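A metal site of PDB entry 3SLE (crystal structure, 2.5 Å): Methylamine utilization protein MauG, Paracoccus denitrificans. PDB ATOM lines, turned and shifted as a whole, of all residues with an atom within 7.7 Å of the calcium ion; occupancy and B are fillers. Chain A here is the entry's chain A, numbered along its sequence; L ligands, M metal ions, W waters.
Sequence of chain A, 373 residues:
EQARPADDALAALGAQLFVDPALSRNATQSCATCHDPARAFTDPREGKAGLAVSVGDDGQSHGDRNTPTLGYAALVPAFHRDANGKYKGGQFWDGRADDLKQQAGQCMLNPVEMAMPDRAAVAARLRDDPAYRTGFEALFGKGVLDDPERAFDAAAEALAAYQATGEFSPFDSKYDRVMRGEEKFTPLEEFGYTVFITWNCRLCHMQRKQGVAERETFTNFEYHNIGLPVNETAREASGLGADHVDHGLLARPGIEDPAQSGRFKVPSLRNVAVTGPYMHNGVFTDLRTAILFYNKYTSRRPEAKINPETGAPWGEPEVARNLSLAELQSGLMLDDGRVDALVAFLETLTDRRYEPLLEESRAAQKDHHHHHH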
ATOM      1  N   ARG A  39     -27.631  26.436  14.489  1.00  0.00           N
ATOM      2  CA  ARG A  39     -26.687  26.593  13.371  1.00  0.00           C
ATOM      3  C   ARG A  39     -25.351  25.927  13.650  1.00  0.00           C
ATOM      4  O   ARG A  39     -24.298  26.513  13.419  1.00  0.00           O
ATOM      5  CB  ARG A  39     -26.453  28.069  13.020  1.00  0.00           C
ATOM      6  CG  ARG A  39     -25.921  28.284  11.613  1.00  0.00           C
ATOM      7  CD  ARG A  39     -25.964  29.747  11.198  1.00  0.00           C
ATOM      8  NE  ARG A  39     -24.725  30.158  10.524  1.00  0.00           N
ATOM      9  CZ  ARG A  39     -24.602  30.334   9.209  1.00  0.00           C
ATOM     10  NH1 ARG A  39     -25.645  30.151   8.412  1.00  0.00           N
ATOM     11  NH2 ARG A  39     -23.446  30.705   8.689  1.00  0.00           N
ATOM     12  N   THR A  42     -22.794  27.986  15.538  1.00  0.00           N
ATOM     13  CA  THR A  42     -22.162  29.204  14.987  1.00  0.00           C
ATOM     14  C   THR A  42     -23.045  30.433  15.129  1.00  0.00           C
ATOM     15  O   THR A  42     -24.122  30.350  15.679  1.00  0.00           O
ATOM     16  CB  THR A  42     -21.724  29.020  13.536  1.00  0.00           C
ATOM     17  OG1 THR A  42     -22.850  28.674  12.725  1.00  0.00           O
ATOM     18  CG2 THR A  42     -20.673  27.920  13.463  1.00  0.00           C
ATOM     19  N   ASP A  43     -22.565  31.569  14.646  1.00  0.00           N
ATOM     20  CA  ASP A  43     -23.312  32.802  14.726  1.00  0.00           C
ATOM     21  C   ASP A  43     -24.085  33.036  13.417  1.00  0.00           C
ATOM     22  O   ASP A  43     -23.450  33.156  12.368  1.00  0.00           O
ATOM     23  CB  ASP A  43     -22.391  33.980  15.090  1.00  0.00           C
ATOM     24  CG  ASP A  43     -23.165  35.248  15.500  1.00  0.00           C
ATOM     25  OD1 ASP A  43     -22.560  36.278  15.849  1.00  0.00           O
ATOM     26  OD2 ASP A  43     -24.406  35.219  15.451  1.00  0.00           O
ATOM     27  N   LEU A  51     -21.943  37.916   8.113  1.00  0.00           N
ATOM     28  CA  LEU A  51     -21.846  36.828   9.102  1.00  0.00           C
ATOM     29  C   LEU A  51     -20.402  36.505   9.478  1.00  0.00           C
ATOM     30  O   LEU A  51     -20.137  35.568  10.250  1.00  0.00           O
ATOM     31  CB  LEU A  51     -22.515  35.579   8.537  1.00  0.00           C
ATOM     32  CG  LEU A  51     -23.978  35.214   8.818  1.00  0.00           C
ATOM     33  CD1 LEU A  51     -24.884  36.439   9.013  1.00  0.00           C
ATOM     34  CD2 LEU A  51     -24.520  34.299   7.689  1.00  0.00           C
ATOM     35  N   ALA A  52     -19.463  37.312   8.963  1.00  0.00           N
ATOM     36  CA  ALA A  52     -18.016  37.085   9.081  1.00  0.00           C
ATOM     37  C   ALA A  52     -17.500  37.121  10.514  1.00  0.00           C
ATOM     38  O   ALA A  52     -16.696  36.262  10.916  1.00  0.00           O
ATOM     39  CB  ALA A  52     -17.249  38.080   8.203  1.00  0.00           C
ATOM     40  N   ASN A  66     -13.847  34.806  12.719  1.00  0.00           N
ATOM     41  CA  ASN A  66     -15.128  34.113  12.540  1.00  0.00           C
ATOM     42  C   ASN A  66     -15.372  33.193  13.717  1.00  0.00           C
ATOM     43  O   ASN A  66     -14.474  32.474  14.170  1.00  0.00           O
ATOM     44  CB  ASN A  66     -15.112  33.331  11.243  1.00  0.00           C
ATOM     45  CG  ASN A  66     -16.458  32.720  10.904  1.00  0.00           C
ATOM     46  OD1 ASN A  66     -16.531  31.517  10.641  1.00  0.00           O
ATOM     47  ND2 ASN A  66     -17.519  33.545  10.848  1.00  0.00           N
ATOM     48  N   THR A  67     -16.571  33.250  14.262  1.00  0.00           N
ATOM     49  CA  THR A  67     -16.968  32.416  15.382  1.00  0.00           C
ATOM     50  C   THR A  67     -17.076  30.964  14.900  1.00  0.00           C
ATOM     51  O   THR A  67     -17.767  30.662  13.929  1.00  0.00           O
ATOM     52  CB  THR A  67     -18.310  32.878  15.870  1.00  0.00           C
ATOM     53  OG1 THR A  67     -18.167  34.195  16.410  1.00  0.00           O
ATOM     54  CG2 THR A  67     -18.846  31.939  16.918  1.00  0.00           C
ATOM     55  N   PRO A  68     -16.365  30.047  15.549  1.00  0.00           N
ATOM     56  CA  PRO A  68     -16.406  28.702  15.016  1.00  0.00           C
ATOM     57  C   PRO A  68     -17.287  27.739  15.821  1.00  0.00           C
ATOM     58  O   PRO A  68     -17.630  28.023  16.996  1.00  0.00           O
ATOM     59  CB  PRO A  68     -14.952  28.275  15.097  1.00  0.00           C
ATOM     60  CG  PRO A  68     -14.472  28.936  16.366  1.00  0.00           C
ATOM     61  CD  PRO A  68     -15.218  30.251  16.451  1.00  0.00           C
ATOM     62  N   THR A  69     -17.628  26.616  15.180  1.00  0.00           N
ATOM     63  CA  THR A  69     -18.513  25.595  15.722  1.00  0.00           C
ATOM     64  C   THR A  69     -17.907  24.961  16.977  1.00  0.00           C
ATOM     65  O   THR A  69     -16.709  24.867  17.081  1.00  0.00           O
ATOM     66  CB  THR A  69     -18.747  24.496  14.666  1.00  0.00           C
ATOM     67  OG1 THR A  69     -19.655  23.565  15.182  1.00  0.00           O
ATOM     68  CG2 THR A  69     -17.406  23.732  14.314  1.00  0.00           C
ATOM     69  N   TRP A  93      -8.749  29.986  17.091  1.00  0.00           N
ATOM     70  CA  TRP A  93      -8.043  29.848  15.844  1.00  0.00           C
ATOM     71  C   TRP A  93      -6.527  29.954  15.997  1.00  0.00           C
ATOM     72  O   TRP A  93      -5.814  29.531  15.086  1.00  0.00           O
ATOM     73  CB  TRP A  93      -8.504  30.874  14.846  1.00  0.00           C
ATOM     74  CG  TRP A  93      -9.852  30.694  14.274  1.00  0.00           C
ATOM     75  CD1 TRP A  93     -11.005  31.332  14.674  1.00  0.00           C
ATOM     76  CD2 TRP A  93     -10.225  29.875  13.143  1.00  0.00           C
ATOM     77  NE1 TRP A  93     -12.066  30.935  13.880  1.00  0.00           N
ATOM     78  CE2 TRP A  93     -11.622  30.069  12.918  1.00  0.00           C
ATOM     79  CE3 TRP A  93      -9.513  29.015  12.300  1.00  0.00           C
ATOM     80  CZ2 TRP A  93     -12.314  29.425  11.885  1.00  0.00           C
ATOM     81  CZ3 TRP A  93     -10.209  28.371  11.245  1.00  0.00           C
ATOM     82  CH2 TRP A  93     -11.599  28.583  11.057  1.00  0.00           C
ATOM     83  N   ASN A 271     -19.706  19.389   9.823  1.00  0.00           N
ATOM     84  CA  ASN A 271     -20.705  20.488   9.668  1.00  0.00           C
ATOM     85  C   ASN A 271     -20.277  21.715   8.827  1.00  0.00           C
ATOM     86  O   ASN A 271     -20.903  22.789   8.884  1.00  0.00           O
ATOM     87  CB  ASN A 271     -21.247  20.910  11.021  1.00  0.00           C
ATOM     88  CG  ASN A 271     -22.137  19.827  11.629  1.00  0.00           C
ATOM     89  OD1 ASN A 271     -22.961  19.228  10.906  1.00  0.00           O
ATOM     90  ND2 ASN A 271     -21.929  19.505  12.933  1.00  0.00           N
ATOM     91  N   VAL A 272     -19.233  21.570   8.036  1.00  0.00           N
ATOM     92  CA  VAL A 272     -18.702  22.716   7.303  1.00  0.00           C
ATOM     93  C   VAL A 272     -19.752  23.223   6.323  1.00  0.00           C
ATOM     94  O   VAL A 272     -19.836  24.436   6.059  1.00  0.00           O
ATOM     95  CB  VAL A 272     -17.351  22.399   6.563  1.00  0.00           C
ATOM     96  CG1 VAL A 272     -17.592  21.513   5.358  1.00  0.00           C
ATOM     97  CG2 VAL A 272     -16.658  23.671   6.168  1.00  0.00           C
ATOM     98  N   VAL A 274     -22.671  23.867   6.728  1.00  0.00           N
ATOM     99  CA  VAL A 274     -23.653  24.724   7.316  1.00  0.00           C
ATOM    100  C   VAL A 274     -23.079  25.852   8.165  1.00  0.00           C
ATOM    101  O   VAL A 274     -23.819  26.525   8.873  1.00  0.00           O
ATOM    102  CB  VAL A 274     -24.686  23.909   8.126  1.00  0.00           C
ATOM    103  CG1 VAL A 274     -25.395  22.935   7.235  1.00  0.00           C
ATOM    104  CG2 VAL A 274     -24.027  23.179   9.234  1.00  0.00           C
ATOM    105  N   THR A 275     -21.753  26.056   8.113  1.00  0.00           N
ATOM    106  CA  THR A 275     -21.088  26.979   9.064  1.00  0.00           C
ATOM    107  C   THR A 275     -20.289  28.120   8.422  1.00  0.00           C
ATOM    108  O   THR A 275     -19.393  28.710   9.091  1.00  0.00           O
ATOM    109  CB  THR A 275     -20.158  26.246  10.021  1.00  0.00           C
ATOM    110  OG1 THR A 275     -19.233  25.469   9.253  1.00  0.00           O
ATOM    111  CG2 THR A 275     -20.918  25.342  10.925  1.00  0.00           C
ATOM    112  N   GLY A 276     -20.622  28.415   7.168  1.00  0.00           N
ATOM    113  CA  GLY A 276     -20.108  29.606   6.495  1.00  0.00           C
ATOM    114  C   GLY A 276     -20.379  30.872   7.305  1.00  0.00           C
ATOM    115  O   GLY A 276     -21.101  30.860   8.291  1.00  0.00           O
ATOM    116  N   PRO A 277     -19.749  31.975   6.906  1.00  0.00           N
ATOM    117  CA  PRO A 277     -18.716  32.001   5.896  1.00  0.00           C
ATOM    118  C   PRO A 277     -17.440  31.329   6.446  1.00  0.00           C
ATOM    119  O   PRO A 277     -17.423  30.866   7.593  1.00  0.00           O
ATOM    120  CB  PRO A 277     -18.528  33.500   5.659  1.00  0.00           C
ATOM    121  CG  PRO A 277     -18.807  34.107   6.998  1.00  0.00           C
ATOM    122  CD  PRO A 277     -19.953  33.306   7.516  1.00  0.00           C
ATOM    123  N   TYR A 278     -16.368  31.290   5.670  1.00  0.00           N
ATOM    124  CA  TYR A 278     -15.285  30.333   5.946  1.00  0.00           C
ATOM    125  C   TYR A 278     -13.949  30.999   6.204  1.00  0.00           C
ATOM    126  O   TYR A 278     -13.775  32.190   5.910  1.00  0.00           O
ATOM    127  CB  TYR A 278     -15.180  29.295   4.817  1.00  0.00           C
ATOM    128  CG  TYR A 278     -16.486  28.547   4.657  1.00  0.00           C
ATOM    129  CD1 TYR A 278     -17.461  28.959   3.739  1.00  0.00           C
ATOM    130  CD2 TYR A 278     -16.765  27.464   5.470  1.00  0.00           C
ATOM    131  CE1 TYR A 278     -18.685  28.291   3.637  1.00  0.00           C
ATOM    132  CE2 TYR A 278     -17.973  26.781   5.378  1.00  0.00           C
ATOM    133  CZ  TYR A 278     -18.934  27.189   4.461  1.00  0.00           C
ATOM    134  OH  TYR A 278     -20.130  26.512   4.399  1.00  0.00           O
ATOM    135  N   MET A 279     -13.029  30.200   6.762  1.00  0.00           N
ATOM    136  CA  MET A 279     -11.680  30.621   7.171  1.00  0.00           C
ATOM    137  C   MET A 279     -11.757  31.421   8.467  1.00  0.00           C
ATOM    138  O   MET A 279     -12.873  31.840   8.892  1.00  0.00           O
ATOM    139  CB  MET A 279     -10.955  31.423   6.080  1.00  0.00           C
ATOM    140  CG  MET A 279     -10.836  30.674   4.803  1.00  0.00           C
ATOM    141  SD  MET A 279     -10.227  28.999   5.081  1.00  0.00           S
ATOM    142  CE  MET A 279     -10.224  28.349   3.444  1.00  0.00           C
ATOM    143  N   HIS A 280     -10.599  31.635   9.085  1.00  0.00           N
ATOM    144  CA  HIS A 280     -10.534  32.332  10.366  1.00  0.00           C
ATOM    145  C   HIS A 280     -11.148  33.755  10.365  1.00  0.00           C
ATOM    146  O   HIS A 280     -11.483  34.298  11.427  1.00  0.00           O
ATOM    147  CB  HIS A 280      -9.101  32.385  10.859  1.00  0.00           C
ATOM    148  CG  HIS A 280      -8.220  33.295  10.056  1.00  0.00           C
ATOM    149  ND1 HIS A 280      -7.277  32.827   9.153  1.00  0.00           N
ATOM    150  CD2 HIS A 280      -8.106  34.646  10.056  1.00  0.00           C
ATOM    151  CE1 HIS A 280      -6.642  33.857   8.622  1.00  0.00           C
ATOM    152  NE2 HIS A 280      -7.129  34.959   9.138  1.00  0.00           N
ATOM    153  N   GLY A 282     -13.802  34.713   8.143  1.00  0.00           N
ATOM    154  CA  GLY A 282     -15.082  34.691   7.404  1.00  0.00           C
ATOM    155  C   GLY A 282     -15.025  35.293   6.005  1.00  0.00           C
ATOM    156  O   GLY A 282     -16.033  35.773   5.480  1.00  0.00           O
ATOM    157  N   PHE A 284     -14.780  34.098   2.945  1.00  0.00           N
ATOM    158  CA  PHE A 284     -15.502  33.494   1.828  1.00  0.00           C
ATOM    159  C   PHE A 284     -16.891  33.138   2.297  1.00  0.00           C
ATOM    160  O   PHE A 284     -16.995  32.409   3.286  1.00  0.00           O
ATOM    161  CB  PHE A 284     -14.836  32.206   1.355  1.00  0.00           C
ATOM    162  CG  PHE A 284     -13.388  32.346   1.035  1.00  0.00           C
ATOM    163  CD1 PHE A 284     -12.900  33.451   0.312  1.00  0.00           C
ATOM    164  CD2 PHE A 284     -12.501  31.350   1.409  1.00  0.00           C
ATOM    165  CE1 PHE A 284     -11.537  33.554  -0.003  1.00  0.00           C
ATOM    166  CE2 PHE A 284     -11.150  31.435   1.085  1.00  0.00           C
ATOM    167  CZ  PHE A 284     -10.660  32.529   0.384  1.00  0.00           C
HETATM  168 FE1  LIG L   1      -8.237  23.195   4.308  1.00  0.00          FE
HETATM  169  C1  LIG L   1      -9.756  25.619   6.170  1.00  0.00           C
HETATM  170  C2  LIG L   1     -11.124  22.455   2.843  1.00  0.00           C
HETATM  171  C3  LIG L   1      -6.568  21.138   2.113  1.00  0.00           C
HETATM  172  C4  LIG L   1      -5.371  23.439   6.133  1.00  0.00           C
HETATM  173  N1  LIG L   1     -10.040  23.917   4.475  1.00  0.00           N
HETATM  174  C5  LIG L   1     -10.523  24.900   5.315  1.00  0.00           C
HETATM  175  C6  LIG L   1     -11.966  25.086   5.134  1.00  0.00           C
HETATM  176  C7  LIG L   1     -12.333  24.191   4.184  1.00  0.00           C
HETATM  177  C8  LIG L   1     -11.133  23.457   3.778  1.00  0.00           C
HETATM  178  C9  LIG L   1     -13.761  23.950   3.632  1.00  0.00           C
HETATM  179  C10 LIG L   1     -12.895  26.093   5.867  1.00  0.00           C
HETATM  180  C11 LIG L   1     -13.461  25.483   7.174  1.00  0.00           C
HETATM  181  C12 LIG L   1     -14.003  26.523   8.133  1.00  0.00           C
HETATM  182  O1  LIG L   1     -13.747  27.751   7.976  1.00  0.00           O
HETATM  183  O2  LIG L   1     -14.682  26.114   9.113  1.00  0.00           O
HETATM  184  N2  LIG L   1      -8.736  22.022   2.800  1.00  0.00           N
HETATM  185  C13 LIG L   1      -9.990  21.896   2.310  1.00  0.00           C
HETATM  186  C14 LIG L   1      -9.962  21.099   1.115  1.00  0.00           C
HETATM  187  C15 LIG L   1      -8.711  20.733   0.905  1.00  0.00           C
HETATM  188  C16 LIG L   1      -7.914  21.316   1.960  1.00  0.00           C
HETATM  189  C17 LIG L   1     -11.222  20.719   0.295  1.00  0.00           C
HETATM  190  C18 LIG L   1      -8.170  19.862  -0.245  1.00  0.00           C
HETATM  191  C19 LIG L   1      -8.267  20.734  -1.520  1.00  0.00           C
HETATM  192  N3  LIG L   1      -6.360  22.389   4.182  1.00  0.00           N
HETATM  193  C20 LIG L   1      -5.850  21.619   3.154  1.00  0.00           C
HETATM  194  C21 LIG L   1      -4.422  21.438   3.347  1.00  0.00           C
HETATM  195  C22 LIG L   1      -4.068  22.105   4.458  1.00  0.00           C
HETATM  196  C23 LIG L   1      -5.298  22.681   5.014  1.00  0.00           C
HETATM  197  C24 LIG L   1      -3.473  20.687   2.403  1.00  0.00           C
HETATM  198  C25 LIG L   1      -2.657  22.205   5.104  1.00  0.00           C
HETATM  199  C26 LIG L   1      -1.496  22.372   4.106  1.00  0.00           C
HETATM  200  N4  LIG L   1      -7.667  24.348   5.897  1.00  0.00           N
HETATM  201  C27 LIG L   1      -6.393  24.332   6.430  1.00  0.00           C
HETATM  202  C28 LIG L   1      -6.296  25.407   7.405  1.00  0.00           C
HETATM  203  C29 LIG L   1      -7.670  26.050   7.413  1.00  0.00           C
HETATM  204  C30 LIG L   1      -8.443  25.323   6.472  1.00  0.00           C
HETATM  205  C31 LIG L   1      -5.079  25.800   8.247  1.00  0.00           C
HETATM  206  C32 LIG L   1      -8.092  27.255   8.220  1.00  0.00           C
HETATM  207  C33 LIG L   1      -7.084  28.302   7.757  1.00  0.00           C
HETATM  208  C34 LIG L   1      -7.537  29.655   8.227  1.00  0.00           C
HETATM  209  O3  LIG L   1      -8.735  29.828   8.570  1.00  0.00           O
HETATM  210  O4  LIG L   1      -6.677  30.552   8.269  1.00  0.00           O
HETATM  211 CA    CA M   1     -17.410  29.572   9.761  1.00  0.00          CA
HETATM  212  O   HOH W   1     -15.076  29.073   9.542  1.00  0.00           O
HETATM  213  O   HOH W   2     -17.033  27.326   9.276  1.00  0.00           O
HETATM  214  O   HOH W   3     -18.028  29.029  11.993  1.00  0.00           O
HETATM  215  O   HOH W   4     -19.553  31.207  10.495  1.00  0.00           O
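The backbone NH (N) of Met 279 sits at hydrogen-bond distance from an oxygen (O1) of the ligand (2.8 Å). An oxygen (O3) of the ligand sits at hydrogen-bond distance from the backbone NH (N) of His 280. O4 of the ligand lies within hydrogen-bond range of ND1 of His 280 (2.5 Å).
The calcium ion is bound by the backbone carbonyl oxygen (O) of Thr 275 (2.3 Å), the side-chain amide oxygen (OD1) of Asn 66 (2.3 Å), water W2 (2.3 Å), water W3 (2.4 Å), water W1 (2.4 Å), the backbone carbonyl oxygen (O) of Pro 277 (2.5 Å) and water W4 (2.8 Å).
Water W2 bridges an oxygen (O2) of the ligand (2.7 Å) and the side-chain hydroxyl of Thr 275 (2.9 Å). Water W4 bridges O of Gly 276 (2.7 Å) and ND2 of Asn 66 (3.1 Å).
The side-chain hydroxyl (OG1) of Thr 275 is in hydrogen-bond range of the backbone carbonyl oxygen (O) of Val 272 (3.4 Å). The side-chain hydroxyl (OG1) of Thr 275 lies within hydrogen-bond range of the backbone carbonyl oxygen (O) of Asn 271 (3.2 Å). The backbone carbonyl oxygen (O) of Asn 66 lies within hydrogen-bond range of the indole nitrogen (NE1) of Trp 93 (2.9 Å). O of Leu 51 lies within hydrogen-bond range of ND2 of Asn 66, at 3.4 Å. The side-chain amide nitrogen (ND2) of Asn 66 is in hydrogen-bond range of the backbone carbonyl oxygen (O) of Ala 52. N of Asn 66 lies within hydrogen-bond range of O of His 280 (2.7 Å).
Along chain A the residues within 4 Å of the calcium ion span positions 66 to 277. The nearest printed residue that does not touch the calcium ion is Gly 276 (4.1 Å).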
